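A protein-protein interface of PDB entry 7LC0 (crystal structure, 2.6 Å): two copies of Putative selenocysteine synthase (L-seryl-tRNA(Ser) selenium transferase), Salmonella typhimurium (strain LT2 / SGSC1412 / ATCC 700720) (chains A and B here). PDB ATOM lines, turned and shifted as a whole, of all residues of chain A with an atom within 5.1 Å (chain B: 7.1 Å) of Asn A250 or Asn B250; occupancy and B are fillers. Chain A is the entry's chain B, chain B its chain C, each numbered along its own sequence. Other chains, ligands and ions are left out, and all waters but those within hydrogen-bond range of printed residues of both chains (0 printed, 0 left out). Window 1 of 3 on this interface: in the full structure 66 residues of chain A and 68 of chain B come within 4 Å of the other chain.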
ATOM      1  N   THR A  37     -39.887   4.164 -16.430  1.00  0.00           N
ATOM      2  CA  THR A  37     -38.723   4.801 -17.034  1.00  0.00           C
ATOM      3  C   THR A  37     -38.876   4.910 -18.546  1.00  0.00           C
ATOM      4  O   THR A  37     -38.497   5.926 -19.143  1.00  0.00           O
ATOM      5  CB  THR A  37     -37.459   4.021 -16.673  1.00  0.00           C
ATOM      6  OG1 THR A  37     -37.305   3.993 -15.248  1.00  0.00           O
ATOM      7  CG2 THR A  37     -36.227   4.662 -17.296  1.00  0.00           C
ATOM      8  N   PRO A 218     -33.032   2.494 -11.360  1.00  0.00           N
ATOM      9  CA  PRO A 218     -32.066   2.858 -12.398  1.00  0.00           C
ATOM     10  C   PRO A 218     -31.057   3.848 -11.837  1.00  0.00           C
ATOM     11  O   PRO A 218     -31.287   4.492 -10.811  1.00  0.00           O
ATOM     12  CB  PRO A 218     -32.933   3.485 -13.498  1.00  0.00           C
ATOM     13  CG  PRO A 218     -34.234   3.823 -12.829  1.00  0.00           C
ATOM     14  CD  PRO A 218     -34.416   2.783 -11.771  1.00  0.00           C
ATOM     15  N   THR A 219     -29.914   3.947 -12.519  1.00  0.00           N
ATOM     16  CA  THR A 219     -28.787   4.745 -12.046  1.00  0.00           C
ATOM     17  C   THR A 219     -29.219   6.133 -11.591  1.00  0.00           C
ATOM     18  O   THR A 219     -29.493   7.011 -12.416  1.00  0.00           O
ATOM     19  CB  THR A 219     -27.724   4.863 -13.135  1.00  0.00           C
ATOM     20  OG1 THR A 219     -27.276   3.552 -13.493  1.00  0.00           O
ATOM     21  CG2 THR A 219     -26.544   5.676 -12.634  1.00  0.00           C
ATOM     22  N   SER A 220     -29.287   6.330 -10.277  1.00  0.00           N
ATOM     23  CA  SER A 220     -29.796   7.571  -9.718  1.00  0.00           C
ATOM     24  C   SER A 220     -29.358   7.687  -8.268  1.00  0.00           C
ATOM     25  O   SER A 220     -29.006   6.697  -7.621  1.00  0.00           O
ATOM     26  CB  SER A 220     -31.323   7.644  -9.815  1.00  0.00           C
ATOM     27  OG  SER A 220     -31.927   6.597  -9.075  1.00  0.00           O
ATOM     28  N   ILE A 246     -28.232  13.434 -14.820  1.00  0.00           N
ATOM     29  CA  ILE A 246     -29.238  12.383 -14.844  1.00  0.00           C
ATOM     30  C   ILE A 246     -30.432  12.910 -15.624  1.00  0.00           C
ATOM     31  O   ILE A 246     -30.837  14.065 -15.450  1.00  0.00           O
ATOM     32  CB  ILE A 246     -29.653  11.933 -13.426  1.00  0.00           C
ATOM     33  CG1 ILE A 246     -30.767  10.888 -13.505  1.00  0.00           C
ATOM     34  CG2 ILE A 246     -30.078  13.124 -12.576  1.00  0.00           C
ATOM     35  CD1 ILE A 246     -31.214  10.370 -12.164  1.00  0.00           C
ATOM     36  N   GLY A 247     -30.983  12.072 -16.502  1.00  0.00           N
ATOM     37  CA  GLY A 247     -32.061  12.489 -17.371  1.00  0.00           C
ATOM     38  C   GLY A 247     -33.430  12.270 -16.763  1.00  0.00           C
ATOM     39  O   GLY A 247     -33.587  11.750 -15.660  1.00  0.00           O
ATOM     40  N   LYS A 248     -34.445  12.685 -17.522  1.00  0.00           N
ATOM     41  CA  LYS A 248     -35.818  12.576 -17.045  1.00  0.00           C
ATOM     42  C   LYS A 248     -36.237  11.126 -16.851  1.00  0.00           C
ATOM     43  O   LYS A 248     -37.062  10.834 -15.977  1.00  0.00           O
ATOM     44  CB  LYS A 248     -36.762  13.283 -18.018  1.00  0.00           C
ATOM     45  CG  LYS A 248     -36.533  12.916 -19.475  1.00  0.00           C
ATOM     46  CD  LYS A 248     -37.414  13.741 -20.397  1.00  0.00           C
ATOM     47  CE  LYS A 248     -37.059  13.504 -21.853  1.00  0.00           C
ATOM     48  NZ  LYS A 248     -37.209  12.074 -22.240  1.00  0.00           N
ATOM     49  N   GLU A 249     -35.678  10.204 -17.638  1.00  0.00           N
ATOM     50  CA  GLU A 249     -36.113   8.813 -17.553  1.00  0.00           C
ATOM     51  C   GLU A 249     -35.696   8.178 -16.231  1.00  0.00           C
ATOM     52  O   GLU A 249     -36.464   7.412 -15.638  1.00  0.00           O
ATOM     53  CB  GLU A 249     -35.575   8.011 -18.742  1.00  0.00           C
ATOM     54  CG  GLU A 249     -34.068   7.775 -18.759  1.00  0.00           C
ATOM     55  CD  GLU A 249     -33.278   8.985 -19.218  1.00  0.00           C
ATOM     56  OE1 GLU A 249     -33.891  10.038 -19.497  1.00  0.00           O
ATOM     57  OE2 GLU A 249     -32.038   8.880 -19.305  1.00  0.00           O
ATOM     58  N   ASN A 250     -34.496   8.491 -15.743  1.00  0.00           N
ATOM     59  CA  ASN A 250     -34.036   7.935 -14.479  1.00  0.00           C
ATOM     60  C   ASN A 250     -34.478   8.754 -13.276  1.00  0.00           C
ATOM     61  O   ASN A 250     -34.471   8.233 -12.154  1.00  0.00           O
ATOM     62  CB  ASN A 250     -32.511   7.796 -14.479  1.00  0.00           C
ATOM     63  CG  ASN A 250     -32.027   6.695 -15.406  1.00  0.00           C
ATOM     64  OD1 ASN A 250     -32.796   5.822 -15.807  1.00  0.00           O
ATOM     65  ND2 ASN A 250     -30.744   6.728 -15.743  1.00  0.00           N
ATOM     66  N   MET A 251     -34.858  10.013 -13.477  1.00  0.00           N
ATOM     67  CA  MET A 251     -35.469  10.796 -12.410  1.00  0.00           C
ATOM     68  C   MET A 251     -36.817  10.190 -12.047  1.00  0.00           C
ATOM     69  O   MET A 251     -37.110   9.945 -10.877  1.00  0.00           O
ATOM     70  CB  MET A 251     -35.641  12.257 -12.828  1.00  0.00           C
ATOM     71  CG  MET A 251     -34.356  13.059 -12.873  1.00  0.00           C
ATOM     72  SD  MET A 251     -34.708  14.951 -13.196  1.00  0.00           S
ATOM     73  CE  MET A 251     -33.908  15.128 -14.963  1.00  0.00           C
ATOM     74  N   VAL A 252     -37.638   9.950 -13.071  1.00  0.00           N
ATOM     75  CA  VAL A 252     -38.929   9.308 -12.854  1.00  0.00           C
ATOM     76  C   VAL A 252     -38.733   7.871 -12.386  1.00  0.00           C
ATOM     77  O   VAL A 252     -39.479   7.374 -11.532  1.00  0.00           O
ATOM     78  CB  VAL A 252     -39.782   9.381 -14.133  1.00  0.00           C
ATOM     79  CG1 VAL A 252     -41.109   8.678 -13.925  1.00  0.00           C
ATOM     80  CG2 VAL A 252     -40.005  10.829 -14.540  1.00  0.00           C
ATOM     81  N   GLY A 253     -37.725   7.184 -12.928  1.00  0.00           N
ATOM     82  CA  GLY A 253     -37.451   5.823 -12.501  1.00  0.00           C
ATOM     83  C   GLY A 253     -37.095   5.722 -11.032  1.00  0.00           C
ATOM     84  O   GLY A 253     -37.414   4.724 -10.381  1.00  0.00           O
ATOM     85  N   LEU A 254     -36.438   6.748 -10.488  1.00  0.00           N
ATOM     86  CA  LEU A 254     -36.119   6.746  -9.064  1.00  0.00           C
ATOM     87  C   LEU A 254     -37.373   6.922  -8.218  1.00  0.00           C
ATOM     88  O   LEU A 254     -37.524   6.268  -7.179  1.00  0.00           O
ATOM     89  CB  LEU A 254     -35.103   7.845  -8.753  1.00  0.00           C
ATOM     90  CG  LEU A 254     -34.779   8.070  -7.275  1.00  0.00           C
ATOM     91  CD1 LEU A 254     -34.200   6.810  -6.648  1.00  0.00           C
ATOM     92  CD2 LEU A 254     -33.826   9.242  -7.107  1.00  0.00           C
ATOM     93  N   MET B  34     -35.858   1.700 -25.509  1.00  0.00           N
ATOM     94  CA  MET B  34     -36.136   1.568 -24.085  1.00  0.00           C
ATOM     95  C   MET B  34     -36.423   0.119 -23.708  1.00  0.00           C
ATOM     96  O   MET B  34     -36.207  -0.285 -22.566  1.00  0.00           O
ATOM     97  CB  MET B  34     -37.308   2.462 -23.677  1.00  0.00           C
ATOM     98  CG  MET B  34     -36.974   3.939 -23.681  1.00  0.00           C
ATOM     99  SD  MET B  34     -35.352   4.312 -22.665  1.00  0.00           S
ATOM    100  CE  MET B  34     -35.885   3.558 -20.946  1.00  0.00           C
ATOM    101  N   THR B  37     -33.182  -1.055 -23.089  1.00  0.00           N
ATOM    102  CA  THR B  37     -32.743  -0.427 -21.847  1.00  0.00           C
ATOM    103  C   THR B  37     -33.385  -1.095 -20.637  1.00  0.00           C
ATOM    104  O   THR B  37     -32.728  -1.295 -19.609  1.00  0.00           O
ATOM    105  CB  THR B  37     -33.070   1.066 -21.873  1.00  0.00           C
ATOM    106  OG1 THR B  37     -32.410   1.681 -22.987  1.00  0.00           O
ATOM    107  CG2 THR B  37     -32.614   1.738 -20.585  1.00  0.00           C
ATOM    108  N   ALA B  40     -31.825  -4.520 -19.997  1.00  0.00           N
ATOM    109  CA  ALA B  40     -30.494  -4.374 -19.422  1.00  0.00           C
ATOM    110  C   ALA B  40     -30.557  -4.008 -17.946  1.00  0.00           C
ATOM    111  O   ALA B  40     -29.681  -4.408 -17.171  1.00  0.00           O
ATOM    112  CB  ALA B  40     -29.699  -3.325 -20.196  1.00  0.00           C
ATOM    113  N   ALA B  41     -31.579  -3.255 -17.538  1.00  0.00           N
ATOM    114  CA  ALA B  41     -31.711  -2.867 -16.142  1.00  0.00           C
ATOM    115  C   ALA B  41     -32.263  -3.986 -15.272  1.00  0.00           C
ATOM    116  O   ALA B  41     -32.175  -3.897 -14.042  1.00  0.00           O
ATOM    117  CB  ALA B  41     -32.606  -1.633 -16.020  1.00  0.00           C
ATOM    118  N   ILE B  69     -18.175   4.797 -23.174  1.00  0.00           N
ATOM    119  CA  ILE B  69     -19.474   5.430 -22.969  1.00  0.00           C
ATOM    120  C   ILE B  69     -19.462   6.197 -21.654  1.00  0.00           C
ATOM    121  O   ILE B  69     -19.016   5.682 -20.621  1.00  0.00           O
ATOM    122  CB  ILE B  69     -20.599   4.383 -22.992  1.00  0.00           C
ATOM    123  CG1 ILE B  69     -20.669   3.709 -24.363  1.00  0.00           C
ATOM    124  CG2 ILE B  69     -21.933   5.022 -22.650  1.00  0.00           C
ATOM    125  CD1 ILE B  69     -21.862   2.794 -24.533  1.00  0.00           C
ATOM    126  N   THR B  70     -19.952   7.431 -21.690  1.00  0.00           N
ATOM    127  CA  THR B  70     -20.035   8.303 -20.527  1.00  0.00           C
ATOM    128  C   THR B  70     -21.497   8.650 -20.249  1.00  0.00           C
ATOM    129  O   THR B  70     -22.407   8.233 -20.969  1.00  0.00           O
ATOM    130  CB  THR B  70     -19.209   9.574 -20.738  1.00  0.00           C
ATOM    131  OG1 THR B  70     -19.748  10.317 -21.838  1.00  0.00           O
ATOM    132  CG2 THR B  70     -17.759   9.222 -21.037  1.00  0.00           C
ATOM    133  N   SER B  71     -21.716   9.428 -19.188  1.00  0.00           N
ATOM    134  CA  SER B  71     -23.074   9.824 -18.833  1.00  0.00           C
ATOM    135  C   SER B  71     -23.587  10.960 -19.708  1.00  0.00           C
ATOM    136  O   SER B  71     -24.799  11.071 -19.922  1.00  0.00           O
ATOM    137  CB  SER B  71     -23.138  10.231 -17.359  1.00  0.00           C
ATOM    138  OG  SER B  71     -22.422  11.431 -17.126  1.00  0.00           O
ATOM    139  N   ALA B 217     -31.031   9.094 -27.676  1.00  0.00           N
ATOM    140  CA  ALA B 217     -30.730   8.011 -26.756  1.00  0.00           C
ATOM    141  C   ALA B 217     -31.130   8.386 -25.338  1.00  0.00           C
ATOM    142  O   ALA B 217     -31.322   9.566 -25.025  1.00  0.00           O
ATOM    143  CB  ALA B 217     -29.238   7.684 -26.802  1.00  0.00           C
ATOM    144  N   PRO B 218     -31.277   7.403 -24.449  1.00  0.00           N
ATOM    145  CA  PRO B 218     -31.332   7.723 -23.020  1.00  0.00           C
ATOM    146  C   PRO B 218     -30.046   8.417 -22.597  1.00  0.00           C
ATOM    147  O   PRO B 218     -29.017   8.331 -23.271  1.00  0.00           O
ATOM    148  CB  PRO B 218     -31.488   6.353 -22.345  1.00  0.00           C
ATOM    149  CG  PRO B 218     -31.051   5.359 -23.377  1.00  0.00           C
ATOM    150  CD  PRO B 218     -31.431   5.959 -24.693  1.00  0.00           C
ATOM    151  N   THR B 219     -30.123   9.124 -21.468  1.00  0.00           N
ATOM    152  CA  THR B 219     -29.037   9.990 -21.020  1.00  0.00           C
ATOM    153  C   THR B 219     -27.688   9.285 -21.066  1.00  0.00           C
ATOM    154  O   THR B 219     -27.395   8.424 -20.231  1.00  0.00           O
ATOM    155  CB  THR B 219     -29.314  10.501 -19.610  1.00  0.00           C
ATOM    156  OG1 THR B 219     -30.560  11.204 -19.613  1.00  0.00           O
ATOM    157  CG2 THR B 219     -28.206  11.442 -19.156  1.00  0.00           C
ATOM    158  N   SER B 220     -26.873   9.643 -22.053  1.00  0.00           N
ATOM    159  CA  SER B 220     -25.599   8.976 -22.277  1.00  0.00           C
ATOM    160  C   SER B 220     -24.731   9.856 -23.163  1.00  0.00           C
ATOM    161  O   SER B 220     -25.198  10.814 -23.782  1.00  0.00           O
ATOM    162  CB  SER B 220     -25.798   7.597 -22.915  1.00  0.00           C
ATOM    163  OG  SER B 220     -26.432   7.708 -24.177  1.00  0.00           O
ATOM    164  N   GLY B 221     -23.449   9.510 -23.205  1.00  0.00           N
ATOM    165  CA  GLY B 221     -22.483  10.120 -24.097  1.00  0.00           C
ATOM    166  C   GLY B 221     -21.342   9.146 -24.268  1.00  0.00           C
ATOM    167  O   GLY B 221     -21.248   8.143 -23.558  1.00  0.00           O
ATOM    168  N   LYS B 245     -21.591   9.005 -13.287  1.00  0.00           N
ATOM    169  CA  LYS B 245     -21.900   7.597 -13.484  1.00  0.00           C
ATOM    170  C   LYS B 245     -22.955   7.395 -14.563  1.00  0.00           C
ATOM    171  O   LYS B 245     -23.932   8.143 -14.653  1.00  0.00           O
ATOM    172  CB  LYS B 245     -22.381   6.985 -12.167  1.00  0.00           C
ATOM    173  CG  LYS B 245     -22.942   5.579 -12.285  1.00  0.00           C
ATOM    174  CD  LYS B 245     -21.849   4.526 -12.283  1.00  0.00           C
ATOM    175  CE  LYS B 245     -22.419   3.155 -12.610  1.00  0.00           C
ATOM    176  NZ  LYS B 245     -23.634   2.849 -11.799  1.00  0.00           N
ATOM    177  N   ILE B 246     -22.743   6.371 -15.388  1.00  0.00           N
ATOM    178  CA  ILE B 246     -23.765   5.840 -16.280  1.00  0.00           C
ATOM    179  C   ILE B 246     -23.865   4.342 -16.026  1.00  0.00           C
ATOM    180  O   ILE B 246     -22.842   3.658 -15.905  1.00  0.00           O
ATOM    181  CB  ILE B 246     -23.460   6.128 -17.763  1.00  0.00           C
ATOM    182  CG1 ILE B 246     -24.495   5.439 -18.652  1.00  0.00           C
ATOM    183  CG2 ILE B 246     -22.042   5.697 -18.123  1.00  0.00           C
ATOM    184  CD1 ILE B 246     -24.393   5.796 -20.109  1.00  0.00           C
ATOM    185  N   GLY B 247     -25.095   3.838 -15.923  1.00  0.00           N
ATOM    186  CA  GLY B 247     -25.323   2.457 -15.564  1.00  0.00           C
ATOM    187  C   GLY B 247     -25.424   1.542 -16.767  1.00  0.00           C
ATOM    188  O   GLY B 247     -25.284   1.949 -17.918  1.00  0.00           O
ATOM    189  N   LYS B 248     -25.684   0.267 -16.470  1.00  0.00           N
ATOM    190  CA  LYS B 248     -25.756  -0.748 -17.514  1.00  0.00           C
ATOM    191  C   LYS B 248     -26.950  -0.533 -18.437  1.00  0.00           C
ATOM    192  O   LYS B 248     -26.912  -0.952 -19.600  1.00  0.00           O
ATOM    193  CB  LYS B 248     -25.818  -2.137 -16.877  1.00  0.00           C
ATOM    194  CG  LYS B 248     -27.056  -2.363 -16.023  1.00  0.00           C
ATOM    195  CD  LYS B 248     -26.846  -3.475 -15.010  1.00  0.00           C
ATOM    196  CE  LYS B 248     -28.130  -3.755 -14.240  1.00  0.00           C
ATOM    197  NZ  LYS B 248     -28.776  -2.506 -13.743  1.00  0.00           N
ATOM    198  N   GLU B 249     -28.010   0.119 -17.950  1.00  0.00           N
ATOM    199  CA  GLU B 249     -29.217   0.263 -18.761  1.00  0.00           C
ATOM    200  C   GLU B 249     -29.023   1.288 -19.874  1.00  0.00           C
ATOM    201  O   GLU B 249     -29.493   1.082 -20.999  1.00  0.00           O
ATOM    202  CB  GLU B 249     -30.412   0.634 -17.878  1.00  0.00           C
ATOM    203  CG  GLU B 249     -30.355   2.012 -17.235  1.00  0.00           C
ATOM    204  CD  GLU B 249     -29.501   2.043 -15.986  1.00  0.00           C
ATOM    205  OE1 GLU B 249     -28.989   0.976 -15.585  1.00  0.00           O
ATOM    206  OE2 GLU B 249     -29.348   3.136 -15.403  1.00  0.00           O
ATOM    207  N   ASN B 250     -28.325   2.387 -19.592  1.00  0.00           N
ATOM    208  CA  ASN B 250     -28.129   3.431 -20.588  1.00  0.00           C
ATOM    209  C   ASN B 250     -26.934   3.177 -21.493  1.00  0.00           C
ATOM    210  O   ASN B 250     -26.884   3.728 -22.600  1.00  0.00           O
ATOM    211  CB  ASN B 250     -27.981   4.791 -19.901  1.00  0.00           C
ATOM    212  CG  ASN B 250     -29.303   5.332 -19.400  1.00  0.00           C
ATOM    213  OD1 ASN B 250     -30.272   4.589 -19.244  1.00  0.00           O
ATOM    214  ND2 ASN B 250     -29.353   6.636 -19.152  1.00  0.00           N
ATOM    215  N   MET B 251     -25.975   2.369 -21.054  1.00  0.00           N
ATOM    216  CA  MET B 251     -24.879   1.951 -21.919  1.00  0.00           C
ATOM    217  C   MET B 251     -25.430   1.075 -23.037  1.00  0.00           C
ATOM    218  O   MET B 251     -25.065   1.229 -24.203  1.00  0.00           O
ATOM    219  CB  MET B 251     -23.815   1.201 -21.122  1.00  0.00           C
ATOM    220  CG  MET B 251     -23.031   2.076 -20.167  1.00  0.00           C
ATOM    221  SD  MET B 251     -21.928   1.027 -18.958  1.00  0.00           S
ATOM    222  CE  MET B 251     -20.843   0.090 -20.277  1.00  0.00           C
ATOM    223  N   VAL B 252     -26.321   0.155 -22.664  1.00  0.00           N
ATOM    224  CA  VAL B 252     -26.995  -0.672 -23.658  1.00  0.00           C
ATOM    225  C   VAL B 252     -27.966   0.171 -24.474  1.00  0.00           C
ATOM    226  O   VAL B 252     -28.121  -0.033 -25.685  1.00  0.00           O
ATOM    227  CB  VAL B 252     -27.701  -1.858 -22.973  1.00  0.00           C
ATOM    228  CG1 VAL B 252     -28.546  -2.640 -23.970  1.00  0.00           C
ATOM    229  CG2 VAL B 252     -26.677  -2.770 -22.313  1.00  0.00           C
ATOM    230  N   GLY B 253     -28.623   1.137 -23.831  1.00  0.00           N
ATOM    231  CA  GLY B 253     -29.539   2.003 -24.553  1.00  0.00           C
ATOM    232  C   GLY B 253     -28.845   2.822 -25.625  1.00  0.00           C
ATOM    233  O   GLY B 253     -29.403   3.052 -26.700  1.00  0.00           O
ATOM    234  N   LEU B 254     -27.618   3.264 -25.349  1.00  0.00           N
ATOM    235  CA  LEU B 254     -26.871   4.029 -26.341  1.00  0.00           C
ATOM    236  C   LEU B 254     -26.503   3.167 -27.542  1.00  0.00           C
ATOM    237  O   LEU B 254     -26.528   3.640 -28.684  1.00  0.00           O
ATOM    238  CB  LEU B 254     -25.618   4.631 -25.706  1.00  0.00           C
ATOM    239  CG  LEU B 254     -24.700   5.430 -26.633  1.00  0.00           C
ATOM    240  CD1 LEU B 254     -25.451   6.584 -27.278  1.00  0.00           C
ATOM    241  CD2 LEU B 254     -23.492   5.940 -25.870  1.00  0.00           C
ATOM    242  N   VAL B 255     -26.161   1.899 -27.304  1.00  0.00           N
ATOM    243  CA  VAL B 255     -25.798   1.006 -28.401  1.00  0.00           C
ATOM    244  C   VAL B 255     -26.992   0.787 -29.323  1.00  0.00           C
ATOM    245  O   VAL B 255     -26.878   0.883 -30.551  1.00  0.00           O
ATOM    246  CB  VAL B 255     -25.254  -0.325 -27.853  1.00  0.00           C
ATOM    247  CG1 VAL B 255     -25.049  -1.320 -28.981  1.00  0.00           C
ATOM    248  CG2 VAL B 255     -23.950  -0.095 -27.100  1.00  0.00           C
ATOM    249  N   TYR B 256     -28.160   0.500 -28.744  1.00  0.00           N
ATOM    250  CA  TYR B 256     -29.354   0.284 -29.552  1.00  0.00           C
ATOM    251  C   TYR B 256     -29.889   1.578 -30.150  1.00  0.00           C
ATOM    252  O   TYR B 256     -30.585   1.532 -31.170  1.00  0.00           O
ATOM    253  CB  TYR B 256     -30.434  -0.406 -28.719  1.00  0.00           C
ATOM    254  CG  TYR B 256     -30.232  -1.900 -28.612  1.00  0.00           C
ATOM    255  CD1 TYR B 256     -29.341  -2.438 -27.693  1.00  0.00           C
ATOM    256  CD2 TYR B 256     -30.924  -2.772 -29.441  1.00  0.00           C
ATOM    257  CE1 TYR B 256     -29.150  -3.804 -27.600  1.00  0.00           C
ATOM    258  CE2 TYR B 256     -30.741  -4.136 -29.355  1.00  0.00           C
ATOM    259  CZ  TYR B 256     -29.854  -4.647 -28.433  1.00  0.00           C
ATOM    260  OH  TYR B 256     -29.669  -6.007 -28.347  1.00  0.00           O
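OG1 of Thr A219 lies close to N of Gly B247, at 3.3 Å.
OE2 of Glu B249 is in hydrogen-bond range of OG1 of Thr A219.
The side-chain hydroxyl of Thr B219 lies close to the backbone NH of Gly A247 (3.3 Å).
The side-chain carboxylate of Glu A249 lies within hydrogen-bond range of the side-chain hydroxyl of Thr B219.
The side-chain hydroxyl (OG) of Ser B220 lies within hydrogen-bond range of the backbone carbonyl oxygen (O) of Pro B218.
The backbone carbonyl oxygen (O) of Thr B219 sits at hydrogen-bond distance from the side-chain amide nitrogen (ND2) of Asn B250 (2.9 Å).
The side-chain amino group of Lys B248 is in salt-bridge range of the side-chain carboxylate of Glu B249, at 3.9 Å.
CG2 of Thr A37 touches CE of Met B34, at 3.8 Å.
Thr A219 touches Lys B245 (CG2 to CG, 3.6 Å).
Glu A249 touches Pro B218.
Glu A249 touches Asn B250 (OE2 to ND2, 3.5 Å).
Asn A250 touches Glu B249 (ND2 to OE2, 3.9 Å).
Asn A250 touches Asn B250 (ND2 to ND2, 3.7 Å).
Of the printed residues of chain B, Glu A249 touches Pro B218, Thr B219 and Asn B250.
Of chain B, only Glu B249 (3.9 Å) and Asn B250 (3.7 Å) come within 4 Å of Asn A250.
Printed residues of chain A within 4 Å of Thr B219: Gly A247 and Glu A249.
Printed residues of chain A within 4 Å of Glu B249: Thr A219 and Asn A250.
The nearest printed residue of chain A that does not touch Asn B250 is Gly A247 (6.3 Å).
The nearest printed residue of chain A that does not touch Met B34 is Glu A249 (5.0 Å).
Printed residues of chain B that touch a printed residue of chain A: Met B34, Pro B218, Thr B219, Lys B245, Gly B247, Glu B249 and Asn B250.
Printed residues of chain A that touch a printed residue of chain B: Thr A37, Thr A219, Gly A247, Glu A249 and Asn A250.
Among the printed residues, no Asp or Glu carboxylate lies within 4 Å of a Lys or Arg side-chain nitrogen of the other chain.
Thr A219 touches Gly B247, and with the chains exchanged Gly A247 touches Thr B219.
Thr A219 touches Glu B249, and with the chains exchanged Glu A249 touches Thr B219.
Glu A249 touches Asn B250, and with the chains exchanged Asn A250 touches Glu B249.
Asn B250 touches its own counterpart, Asn A250.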
